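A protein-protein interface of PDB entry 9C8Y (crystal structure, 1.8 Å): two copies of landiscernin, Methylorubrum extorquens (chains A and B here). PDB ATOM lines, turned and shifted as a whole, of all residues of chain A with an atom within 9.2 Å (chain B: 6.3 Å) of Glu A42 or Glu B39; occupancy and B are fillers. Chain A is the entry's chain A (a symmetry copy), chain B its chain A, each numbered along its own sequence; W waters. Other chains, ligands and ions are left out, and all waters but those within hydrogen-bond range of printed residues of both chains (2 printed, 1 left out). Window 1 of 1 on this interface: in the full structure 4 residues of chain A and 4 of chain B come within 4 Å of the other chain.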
ATOM      1  N   CYS A   6      -7.752  14.767  -9.442  1.00  0.00           N
ATOM      2  CA  CYS A   6      -7.409  14.094  -8.197  1.00  0.00           C
ATOM      3  C   CYS A   6      -7.888  12.650  -8.209  1.00  0.00           C
ATOM      4  O   CYS A   6      -7.120  11.728  -7.908  1.00  0.00           O
ATOM      5  CB  CYS A   6      -7.999  14.862  -7.016  1.00  0.00           C
ATOM      6  SG  CYS A   6      -7.976  13.978  -5.457  1.00  0.00           S
ATOM      7  N   LYS A  34      -2.391   8.107   1.234  1.00  0.00           N
ATOM      8  CA  LYS A  34      -3.414   8.381   2.235  1.00  0.00           C
ATOM      9  C   LYS A  34      -3.596   9.878   2.457  1.00  0.00           C
ATOM     10  O   LYS A  34      -4.724  10.325   2.696  1.00  0.00           O
ATOM     11  CB  LYS A  34      -3.091   7.662   3.544  1.00  0.00           C
ATOM     12  CG  LYS A  34      -3.251   6.151   3.420  1.00  0.00           C
ATOM     13  CD  LYS A  34      -3.415   5.451   4.755  1.00  0.00           C
ATOM     14  CE  LYS A  34      -2.208   5.631   5.622  1.00  0.00           C
ATOM     15  NZ  LYS A  34      -2.111   4.561   6.665  1.00  0.00           N
ATOM     16  N   ILE A  35      -2.518  10.664   2.371  1.00  0.00           N
ATOM     17  CA  ILE A  35      -2.650  12.122   2.408  1.00  0.00           C
ATOM     18  C   ILE A  35      -3.492  12.611   1.231  1.00  0.00           C
ATOM     19  O   ILE A  35      -4.393  13.436   1.398  1.00  0.00           O
ATOM     20  CB  ILE A  35      -1.265  12.795   2.424  1.00  0.00           C
ATOM     21  CG1 ILE A  35      -0.536  12.534   3.738  1.00  0.00           C
ATOM     22  CG2 ILE A  35      -1.386  14.290   2.211  1.00  0.00           C
ATOM     23  CD1 ILE A  35      -1.168  13.206   4.912  1.00  0.00           C
ATOM     24  N   ALA A  36      -3.202  12.127   0.018  1.00  0.00           N
ATOM     25  CA  ALA A  36      -3.989  12.517  -1.147  1.00  0.00           C
ATOM     26  C   ALA A  36      -5.461  12.202  -0.938  1.00  0.00           C
ATOM     27  O   ALA A  36      -6.323  13.055  -1.172  1.00  0.00           O
ATOM     28  CB  ALA A  36      -3.473  11.828  -2.406  1.00  0.00           C
ATOM     29  N   GLU A  37      -5.762  10.994  -0.447  1.00  0.00           N
ATOM     30  CA  GLU A  37      -7.153  10.603  -0.226  1.00  0.00           C
ATOM     31  C   GLU A  37      -7.790  11.422   0.894  1.00  0.00           C
ATOM     32  O   GLU A  37      -8.980  11.759   0.818  1.00  0.00           O
ATOM     33  CB  GLU A  37      -7.239   9.106   0.071  1.00  0.00           C
ATOM     34  CG  GLU A  37      -6.862   8.253  -1.128  1.00  0.00           C
ATOM     35  CD  GLU A  37      -6.683   6.788  -0.790  1.00  0.00           C
ATOM     36  OE1 GLU A  37      -6.887   6.420   0.385  1.00  0.00           O
ATOM     37  OE2 GLU A  37      -6.336   6.002  -1.699  1.00  0.00           O
ATOM     38  N   ARG A  38      -7.021  11.748   1.946  1.00  0.00           N
ATOM     39  CA  ARG A  38      -7.531  12.636   2.992  1.00  0.00           C
ATOM     40  C   ARG A  38      -7.914  14.002   2.422  1.00  0.00           C
ATOM     41  O   ARG A  38      -9.005  14.520   2.687  1.00  0.00           O
ATOM     42  CB  ARG A  38      -6.496  12.817   4.105  1.00  0.00           C
ATOM     43  CG  ARG A  38      -6.994  13.776   5.184  1.00  0.00           C
ATOM     44  CD  ARG A  38      -5.911  14.187   6.147  1.00  0.00           C
ATOM     45  NE  ARG A  38      -4.960  15.118   5.553  1.00  0.00           N
ATOM     46  CZ  ARG A  38      -3.761  15.388   6.057  1.00  0.00           C
ATOM     47  NH1 ARG A  38      -3.310  14.780   7.143  1.00  0.00           N
ATOM     48  NH2 ARG A  38      -2.998  16.295   5.460  1.00  0.00           N
ATOM     49  N   GLU A  39      -7.015  14.608   1.653  1.00  0.00           N
ATOM     50  CA  GLU A  39      -7.304  15.910   1.078  1.00  0.00           C
ATOM     51  C   GLU A  39      -8.450  15.832   0.081  1.00  0.00           C
ATOM     52  O   GLU A  39      -9.270  16.751   0.006  1.00  0.00           O
ATOM     53  CB  GLU A  39      -6.043  16.466   0.435  1.00  0.00           C
ATOM     54  CG  GLU A  39      -4.946  16.685   1.458  1.00  0.00           C
ATOM     55  CD  GLU A  39      -5.390  17.627   2.557  1.00  0.00           C
ATOM     56  OE1 GLU A  39      -5.929  18.713   2.233  1.00  0.00           O
ATOM     57  OE2 GLU A  39      -5.211  17.273   3.741  1.00  0.00           O
ATOM     58  N   GLN A  40      -8.538  14.734  -0.679  1.00  0.00           N
ATOM     59  CA  GLN A  40      -9.681  14.535  -1.562  1.00  0.00           C
ATOM     60  C   GLN A  40     -10.977  14.555  -0.767  1.00  0.00           C
ATOM     61  O   GLN A  40     -11.922  15.268  -1.117  1.00  0.00           O
ATOM     62  CB  GLN A  40      -9.542  13.217  -2.327  1.00  0.00           C
ATOM     63  CG  GLN A  40     -10.703  12.914  -3.279  1.00  0.00           C
ATOM     64  CD  GLN A  40     -10.700  11.468  -3.765  1.00  0.00           C
ATOM     65  OE1 GLN A  40     -10.394  10.544  -3.009  1.00  0.00           O
ATOM     66  NE2 GLN A  40     -11.039  11.273  -5.034  1.00  0.00           N
ATOM     67  N   GLY A  41     -11.023  13.802   0.330  1.00  0.00           N
ATOM     68  CA  GLY A  41     -12.199  13.781   1.179  1.00  0.00           C
ATOM     69  C   GLY A  41     -12.509  15.114   1.813  1.00  0.00           C
ATOM     70  O   GLY A  41     -13.662  15.371   2.161  1.00  0.00           O
ATOM     71  N   GLU A  42     -11.514  15.974   1.962  1.00  0.00           N
ATOM     72  CA  GLU A  42     -11.748  17.304   2.506  1.00  0.00           C
ATOM     73  C   GLU A  42     -12.153  18.311   1.442  1.00  0.00           C
ATOM     74  O   GLU A  42     -12.467  19.456   1.786  1.00  0.00           O
ATOM     75  CB  GLU A  42     -10.499  17.782   3.244  1.00  0.00           C
ATOM     76  CG  GLU A  42     -10.211  16.970   4.482  1.00  0.00           C
ATOM     77  CD  GLU A  42      -8.896  17.320   5.145  1.00  0.00           C
ATOM     78  OE1 GLU A  42      -8.199  18.246   4.695  1.00  0.00           O
ATOM     79  OE2 GLU A  42      -8.563  16.643   6.128  1.00  0.00           O
ATOM     80  N   GLY A  43     -12.188  17.905   0.174  1.00  0.00           N
ATOM     81  CA  GLY A  43     -12.521  18.810  -0.904  1.00  0.00           C
ATOM     82  C   GLY A  43     -11.372  19.695  -1.303  1.00  0.00           C
ATOM     83  O   GLY A  43     -11.583  20.719  -1.951  1.00  0.00           O
ATOM     84  N   GLU A  44     -10.156  19.340  -0.908  1.00  0.00           N
ATOM     85  CA  GLU A  44      -8.967  20.101  -1.271  1.00  0.00           C
ATOM     86  C   GLU A  44      -8.224  19.356  -2.373  1.00  0.00           C
ATOM     87  O   GLU A  44      -7.174  18.741  -2.173  1.00  0.00           O
ATOM     88  CB  GLU A  44      -8.094  20.323  -0.051  1.00  0.00           C
ATOM     89  CG  GLU A  44      -8.889  20.785   1.131  1.00  0.00           C
ATOM     90  CD  GLU A  44      -8.041  21.538   2.088  1.00  0.00           C
ATOM     91  OE1 GLU A  44      -7.521  22.591   1.690  1.00  0.00           O
ATOM     92  OE2 GLU A  44      -7.871  21.075   3.227  1.00  0.00           O
ATOM     93  N   PHE A  45      -8.822  19.419  -3.558  1.00  0.00           N
ATOM     94  CA  PHE A  45      -8.348  18.609  -4.664  1.00  0.00           C
ATOM     95  C   PHE A  45      -7.006  19.095  -5.172  1.00  0.00           C
ATOM     96  O   PHE A  45      -6.207  18.291  -5.662  1.00  0.00           O
ATOM     97  CB  PHE A  45      -9.403  18.604  -5.767  1.00  0.00           C
ATOM     98  CG  PHE A  45     -10.764  18.202  -5.271  1.00  0.00           C
ATOM     99  CD1 PHE A  45     -11.010  16.889  -4.878  1.00  0.00           C
ATOM    100  CD2 PHE A  45     -11.779  19.141  -5.149  1.00  0.00           C
ATOM    101  CE1 PHE A  45     -12.255  16.509  -4.398  1.00  0.00           C
ATOM    102  CE2 PHE A  45     -13.029  18.777  -4.665  1.00  0.00           C
ATOM    103  CZ  PHE A  45     -13.273  17.459  -4.287  1.00  0.00           C
ATOM    104  N   ASP A  46      -6.724  20.391  -5.037  1.00  0.00           N
ATOM    105  CA  ASP A  46      -5.399  20.880  -5.381  1.00  0.00           C
ATOM    106  C   ASP A  46      -4.324  20.261  -4.486  1.00  0.00           C
ATOM    107  O   ASP A  46      -3.246  19.889  -4.967  1.00  0.00           O
ATOM    108  CB  ASP A  46      -5.378  22.406  -5.311  1.00  0.00           C
ATOM    109  CG  ASP A  46      -5.995  22.945  -4.035  1.00  0.00           C
ATOM    110  OD1 ASP A  46      -6.251  22.176  -3.089  1.00  0.00           O
ATOM    111  OD2 ASP A  46      -6.237  24.162  -3.976  1.00  0.00           O
ATOM    112  N   GLU A  47      -4.592  20.154  -3.175  1.00  0.00           N
ATOM    113  CA  GLU A  47      -3.633  19.513  -2.276  1.00  0.00           C
ATOM    114  C   GLU A  47      -3.533  18.015  -2.535  1.00  0.00           C
ATOM    115  O   GLU A  47      -2.457  17.430  -2.370  1.00  0.00           O
ATOM    116  CB  GLU A  47      -4.005  19.762  -0.814  1.00  0.00           C
ATOM    117  CG  GLU A  47      -3.854  21.209  -0.358  1.00  0.00           C
ATOM    118  CD  GLU A  47      -2.479  21.782  -0.644  1.00  0.00           C
ATOM    119  OE1 GLU A  47      -1.464  21.071  -0.474  1.00  0.00           O
ATOM    120  OE2 GLU A  47      -2.418  22.955  -1.049  1.00  0.00           O
ATOM    121  N   CYS A  48      -4.637  17.373  -2.922  1.00  0.00           N
ATOM    122  CA  CYS A  48      -4.568  15.982  -3.354  1.00  0.00           C
ATOM    123  C   CYS A  48      -3.578  15.828  -4.515  1.00  0.00           C
ATOM    124  O   CYS A  48      -2.737  14.921  -4.518  1.00  0.00           O
ATOM    125  CB  CYS A  48      -5.970  15.502  -3.754  1.00  0.00           C
ATOM    126  SG  CYS A  48      -6.033  13.992  -4.758  1.00  0.00           S
ATOM    127  N   CYS B   6      -1.457  30.769  13.542  1.00  0.00           N
ATOM    128  CA  CYS B   6      -2.609  29.881  13.605  1.00  0.00           C
ATOM    129  C   CYS B   6      -3.015  29.619  15.048  1.00  0.00           C
ATOM    130  O   CYS B   6      -4.191  29.753  15.407  1.00  0.00           O
ATOM    131  CB  CYS B   6      -2.297  28.578  12.873  1.00  0.00           C
ATOM    132  SG  CYS B   6      -3.466  27.251  13.167  1.00  0.00           S
ATOM    133  N   LYS B  34     -13.566  24.414  13.775  1.00  0.00           N
ATOM    134  CA  LYS B  34     -13.120  23.029  13.706  1.00  0.00           C
ATOM    135  C   LYS B  34     -12.297  22.766  12.450  1.00  0.00           C
ATOM    136  O   LYS B  34     -11.348  21.976  12.498  1.00  0.00           O
ATOM    137  CB  LYS B  34     -14.310  22.075  13.799  1.00  0.00           C
ATOM    138  CG  LYS B  34     -14.933  22.075  15.191  1.00  0.00           C
ATOM    139  CD  LYS B  34     -15.771  20.844  15.475  1.00  0.00           C
ATOM    140  CE  LYS B  34     -16.936  20.743  14.541  1.00  0.00           C
ATOM    141  NZ  LYS B  34     -18.030  19.892  15.108  1.00  0.00           N
ATOM    142  N   ILE B  35     -12.630  23.417  11.331  1.00  0.00           N
ATOM    143  CA  ILE B  35     -11.784  23.338  10.138  1.00  0.00           C
ATOM    144  C   ILE B  35     -10.395  23.903  10.431  1.00  0.00           C
ATOM    145  O   ILE B  35      -9.379  23.299  10.080  1.00  0.00           O
ATOM    146  CB  ILE B  35     -12.444  24.062   8.950  1.00  0.00           C
ATOM    147  CG1 ILE B  35     -13.691  23.324   8.474  1.00  0.00           C
ATOM    148  CG2 ILE B  35     -11.476  24.202   7.794  1.00  0.00           C
ATOM    149  CD1 ILE B  35     -13.395  22.003   7.844  1.00  0.00           C
ATOM    150  N   ALA B  36     -10.326  25.080  11.064  1.00  0.00           N
ATOM    151  CA  ALA B  36      -9.035  25.662  11.413  1.00  0.00           C
ATOM    152  C   ALA B  36      -8.222  24.705  12.270  1.00  0.00           C
ATOM    153  O   ALA B  36      -7.043  24.463  11.992  1.00  0.00           O
ATOM    154  CB  ALA B  36      -9.217  26.994  12.134  1.00  0.00           C
ATOM    155  N   GLU B  37      -8.855  24.112  13.290  1.00  0.00           N
ATOM    156  CA  GLU B  37      -8.146  23.187  14.172  1.00  0.00           C
ATOM    157  C   GLU B  37      -7.746  21.911  13.435  1.00  0.00           C
ATOM    158  O   GLU B  37      -6.670  21.355  13.694  1.00  0.00           O
ATOM    159  CB  GLU B  37      -9.003  22.867  15.398  1.00  0.00           C
ATOM    160  CG  GLU B  37      -9.196  24.073  16.301  1.00  0.00           C
ATOM    161  CD  GLU B  37     -10.246  23.858  17.371  1.00  0.00           C
ATOM    162  OE1 GLU B  37     -10.810  22.747  17.436  1.00  0.00           O
ATOM    163  OE2 GLU B  37     -10.511  24.803  18.147  1.00  0.00           O
ATOM    164  N   ARG B  38      -8.598  21.426  12.516  1.00  0.00           N
ATOM    165  CA  ARG B  38      -8.220  20.281  11.685  1.00  0.00           C
ATOM    166  C   ARG B  38      -6.973  20.584  10.857  1.00  0.00           C
ATOM    167  O   ARG B  38      -6.023  19.793  10.821  1.00  0.00           O
ATOM    168  CB  ARG B  38      -9.369  19.882  10.756  1.00  0.00           C
ATOM    169  CG  ARG B  38      -8.978  18.716   9.851  1.00  0.00           C
ATOM    170  CD  ARG B  38      -9.974  18.473   8.746  1.00  0.00           C
ATOM    171  NE  ARG B  38      -9.915  19.491   7.705  1.00  0.00           N
ATOM    172  CZ  ARG B  38     -10.866  19.697   6.803  1.00  0.00           C
ATOM    173  NH1 ARG B  38     -11.993  19.002   6.809  1.00  0.00           N
ATOM    174  NH2 ARG B  38     -10.681  20.619   5.866  1.00  0.00           N
ATOM    175  N   GLU B  39      -6.969  21.720  10.166  1.00  0.00           N
ATOM    176  CA  GLU B  39      -5.820  22.075   9.351  1.00  0.00           C
ATOM    177  C   GLU B  39      -4.588  22.319  10.209  1.00  0.00           C
ATOM    178  O   GLU B  39      -3.475  21.965   9.810  1.00  0.00           O
ATOM    179  CB  GLU B  39      -6.162  23.293   8.507  1.00  0.00           C
ATOM    180  CG  GLU B  39      -7.295  23.004   7.543  1.00  0.00           C
ATOM    181  CD  GLU B  39      -6.961  21.850   6.622  1.00  0.00           C
ATOM    182  OE1 GLU B  39      -5.855  21.858   6.029  1.00  0.00           O
ATOM    183  OE2 GLU B  39      -7.800  20.932   6.504  1.00  0.00           O
ATOM    184  N   GLN B  40      -4.767  22.904  11.399  1.00  0.00           N
ATOM    185  CA  GLN B  40      -3.650  23.051  12.327  1.00  0.00           C
ATOM    186  C   GLN B  40      -3.048  21.693  12.653  1.00  0.00           C
ATOM    187  O   GLN B  40      -1.831  21.504  12.563  1.00  0.00           O
ATOM    188  CB  GLN B  40      -4.107  23.754  13.606  1.00  0.00           C
ATOM    189  CG  GLN B  40      -3.003  23.949  14.649  1.00  0.00           C
ATOM    190  CD  GLN B  40      -3.551  24.344  16.016  1.00  0.00           C
ATOM    191  OE1 GLN B  40      -4.593  23.848  16.450  1.00  0.00           O
ATOM    192  NE2 GLN B  40      -2.848  25.241  16.696  1.00  0.00           N
ATOM    193  N   GLY B  41      -3.894  20.725  12.998  1.00  0.00           N
ATOM    194  CA  GLY B  41      -3.424  19.384  13.291  1.00  0.00           C
ATOM    195  C   GLY B  41      -2.777  18.701  12.112  1.00  0.00           C
ATOM    196  O   GLY B  41      -1.957  17.803  12.302  1.00  0.00           O
ATOM    197  N   GLU B  42      -3.114  19.110  10.899  1.00  0.00           N
ATOM    198  CA  GLU B  42      -2.484  18.544   9.715  1.00  0.00           C
ATOM    199  C   GLU B  42      -1.191  19.250   9.342  1.00  0.00           C
ATOM    200  O   GLU B  42      -0.512  18.809   8.409  1.00  0.00           O
ATOM    201  CB  GLU B  42      -3.467  18.580   8.546  1.00  0.00           C
ATOM    202  CG  GLU B  42      -4.649  17.667   8.754  1.00  0.00           C
ATOM    203  CD  GLU B  42      -5.714  17.800   7.686  1.00  0.00           C
ATOM    204  OE1 GLU B  42      -5.535  18.563   6.720  1.00  0.00           O
ATOM    205  OE2 GLU B  42      -6.745  17.129   7.833  1.00  0.00           O
ATOM    206  N   GLY B  43      -0.820  20.304  10.068  1.00  0.00           N
ATOM    207  CA  GLY B  43       0.374  21.059   9.755  1.00  0.00           C
ATOM    208  C   GLY B  43       0.180  22.015   8.610  1.00  0.00           C
ATOM    209  O   GLY B  43       1.157  22.470   8.018  1.00  0.00           O
ATOM    210  N   GLU B  44      -1.066  22.313   8.262  1.00  0.00           N
ATOM    211  CA  GLU B  44      -1.371  23.259   7.195  1.00  0.00           C
ATOM    212  C   GLU B  44      -1.817  24.576   7.817  1.00  0.00           C
ATOM    213  O   GLU B  44      -2.992  24.949   7.820  1.00  0.00           O
ATOM    214  CB  GLU B  44      -2.427  22.684   6.271  1.00  0.00           C
ATOM    215  CG  GLU B  44      -2.127  21.267   5.889  1.00  0.00           C
ATOM    216  CD  GLU B  44      -2.769  20.910   4.600  1.00  0.00           C
ATOM    217  OE1 GLU B  44      -2.418  21.537   3.590  1.00  0.00           O
ATOM    218  OE2 GLU B  44      -3.639  20.025   4.592  1.00  0.00           O
ATOM    219  N   PHE B  45      -0.826  25.270   8.367  1.00  0.00           N
ATOM    220  CA  PHE B  45      -1.110  26.448   9.164  1.00  0.00           C
ATOM    221  C   PHE B  45      -1.606  27.594   8.306  1.00  0.00           C
ATOM    222  O   PHE B  45      -2.394  28.419   8.778  1.00  0.00           O
ATOM    223  CB  PHE B  45       0.142  26.831   9.951  1.00  0.00           C
ATOM    224  CG  PHE B  45       0.701  25.688  10.750  1.00  0.00           C
ATOM    225  CD1 PHE B  45       0.016  25.205  11.863  1.00  0.00           C
ATOM    226  CD2 PHE B  45       1.879  25.064  10.364  1.00  0.00           C
ATOM    227  CE1 PHE B  45       0.510  24.136  12.597  1.00  0.00           C
ATOM    228  CE2 PHE B  45       2.383  23.989  11.086  1.00  0.00           C
ATOM    229  CZ  PHE B  45       1.701  23.521  12.206  1.00  0.00           C
ATOM    230  N   GLU B  47      -3.685  27.180   5.767  1.00  0.00           N
ATOM    231  CA  GLU B  47      -5.116  26.911   5.631  1.00  0.00           C
ATOM    232  C   GLU B  47      -5.863  27.162   6.936  1.00  0.00           C
ATOM    233  O   GLU B  47      -7.025  27.579   6.911  1.00  0.00           O
ATOM    234  CB  GLU B  47      -5.360  25.475   5.164  1.00  0.00           C
ATOM    235  CG  GLU B  47      -4.909  25.188   3.736  1.00  0.00           C
ATOM    236  CD  GLU B  47      -5.481  26.163   2.725  1.00  0.00           C
ATOM    237  OE1 GLU B  47      -6.669  26.542   2.833  1.00  0.00           O
ATOM    238  OE2 GLU B  47      -4.731  26.556   1.817  1.00  0.00           O
ATOM    239  N   CYS B  48      -5.227  26.901   8.079  1.00  0.00           N
ATOM    240  CA  CYS B  48      -5.819  27.284   9.356  1.00  0.00           C
ATOM    241  C   CYS B  48      -6.107  28.790   9.384  1.00  0.00           C
ATOM    242  O   CYS B  48      -7.194  29.222   9.785  1.00  0.00           O
ATOM    243  CB  CYS B  48      -4.875  26.881  10.497  1.00  0.00           C
ATOM    244  SG  CYS B  48      -5.180  27.680  12.097  1.00  0.00           S
ATOM    245  N   ALA B  51      -9.205  29.587   7.393  1.00  0.00           N
ATOM    246  CA  ALA B  51     -10.430  29.190   8.075  1.00  0.00           C
ATOM    247  C   ALA B  51     -10.768  30.146   9.205  1.00  0.00           C
ATOM    248  O   ALA B  51     -11.950  30.378   9.487  1.00  0.00           O
ATOM    249  CB  ALA B  51     -10.306  27.765   8.615  1.00  0.00           C
HETATM  250  O   HOH W   1      -0.627  16.509   7.162  1.00  0.00           O
HETATM  251  O   HOH W   2     -13.044  20.423   4.151  1.00  0.00           O
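Water W1 bridges O of Glu B42 (2.6 Å) and NH2 of Arg A38 (2.9 Å). Water W2 lies within hydrogen-bond range of the backbone carbonyl oxygen (O) of Glu A42 (2.6 Å) and the guanidinium group (NH2) of Arg B38 (2.9 Å).
The guanidinium group of Arg B38 lies within salt-bridge range of the side-chain carboxylate of Glu B39. The guanidinium group (NE) of Arg B38 is in salt-bridge range of the side-chain carboxylate (OE2) of Glu B42, 3.96 Å away. The backbone NH (N) of Glu B44 sits at hydrogen-bond distance from the backbone carbonyl oxygen (O) of Glu B39. The guanidinium group (NE) of Arg A38 lies within salt-bridge range of the side-chain carboxylate (OE2) of Glu A39, at 2.8 Å. The backbone carbonyl oxygen (O) of Glu A39 lies within hydrogen-bond range of the backbone NH (N) of Glu A44, 2.9 Å away. SG of Cys A6 forms a disulfide with SG of Cys A48, 2.1 Å away.
Arg A38 touches Glu B44, and with the chains exchanged Glu A44 touches Arg B38. Glu A39 touches Glu B42, and with the chains exchanged Glu A42 touches Glu B39. Glu A39 touches Glu B44, and with the chains exchanged Glu A44 touches Glu B39. Glu B42 touches its own counterpart, Glu A42. Of the 9 pairs that touch across the chains among the printed residues, 9 have their exchanged pair printed and touching as well.
Printed residues of chain B within 4 Å of Glu A42: Arg B38, Glu B39 and Glu B42. Of the printed residues of chain A, Glu B39 touches Glu A42 (3.3 Å) and Glu A44 (3.3 Å). Arg B38 touches two residues of chain A. Gly B41 touches none of the printed residues of chain A. Of chain A, only Arg A38 (3.5 Å), Glu A39 (3.3 Å) and Glu A42 (2.5 Å) come within 4 Å of Glu B42. No residue of chain A comes within 4 Å of Gly B43. Of the printed residues of chain B, Glu A44 touches Arg B38 (3.9 Å) and Glu B39 (3.3 Å). Printed residues of chain B within 4 Å of Glu A39: Glu B42 and Glu B44. Printed residues of chain B within 4 Å of Arg A38: Glu B42 (3.5 Å) and Glu B44 (3.9 Å). Printed residues of chain A within 4 Å of Glu B44: Arg A38 and Glu A39. Asp A46 touches none of the printed residues of chain B. The nearest residue of chain B that does not touch Glu A42 is Glu B44 (4.9 Å). The nearest residue of chain A that does not touch Glu B39 is Glu A39 (4.9 Å). The nearest printed residue of chain A that does not touch Glu B44 is Glu A47 (4.2 Å).
Of the 16 printed residues of chain A, 4 touch a printed residue of chain B. Of the 16 printed residues of chain B, 4 touch a printed residue of chain A. Among the printed residues, Asp or Glu carboxylates within 4 Å of a Lys or Arg side-chain nitrogen of the other chain: Arg A38 with Glu B42 (3.5 Å), Arg A38 with Glu B44 (3.9 Å), Glu A42 with Arg B38 (3.5 Å) and Glu A44 with Arg B38 (3.9 Å).
The side-chain carboxylate (OE2) of Glu A42 lies within salt-bridge range of the guanidinium group (NE) of Arg B38 (3.5 Å). OE2 of Glu A44 lies within salt-bridge range of NH2 of Arg B38 (3.9 Å). The side-chain carboxylate (OE2) of Glu B42 lies within salt-bridge range of the guanidinium group (NE) of Arg A38. OE2 of Glu A42 sits close to OE2 of Glu B42 (2.5 Å). OE2 of Glu B44 lies within salt-bridge range of NH2 of Arg A38, 3.9 Å away. OE2 of Glu A39 sits close to OE1 of Glu B42 (3.3 Å). The side-chain carboxylate (OE2) of Glu A39 sits close to the side-chain carboxylate (OE2) of Glu B44. The side-chain carboxylate (OE1) of Glu A42 sits close to the side-chain carboxylate (OE2) of Glu B39 (3.3 Å). The side-chain carboxylate of Glu B39 sits close to the side-chain carboxylate of Glu A44, 3.3 Å away.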
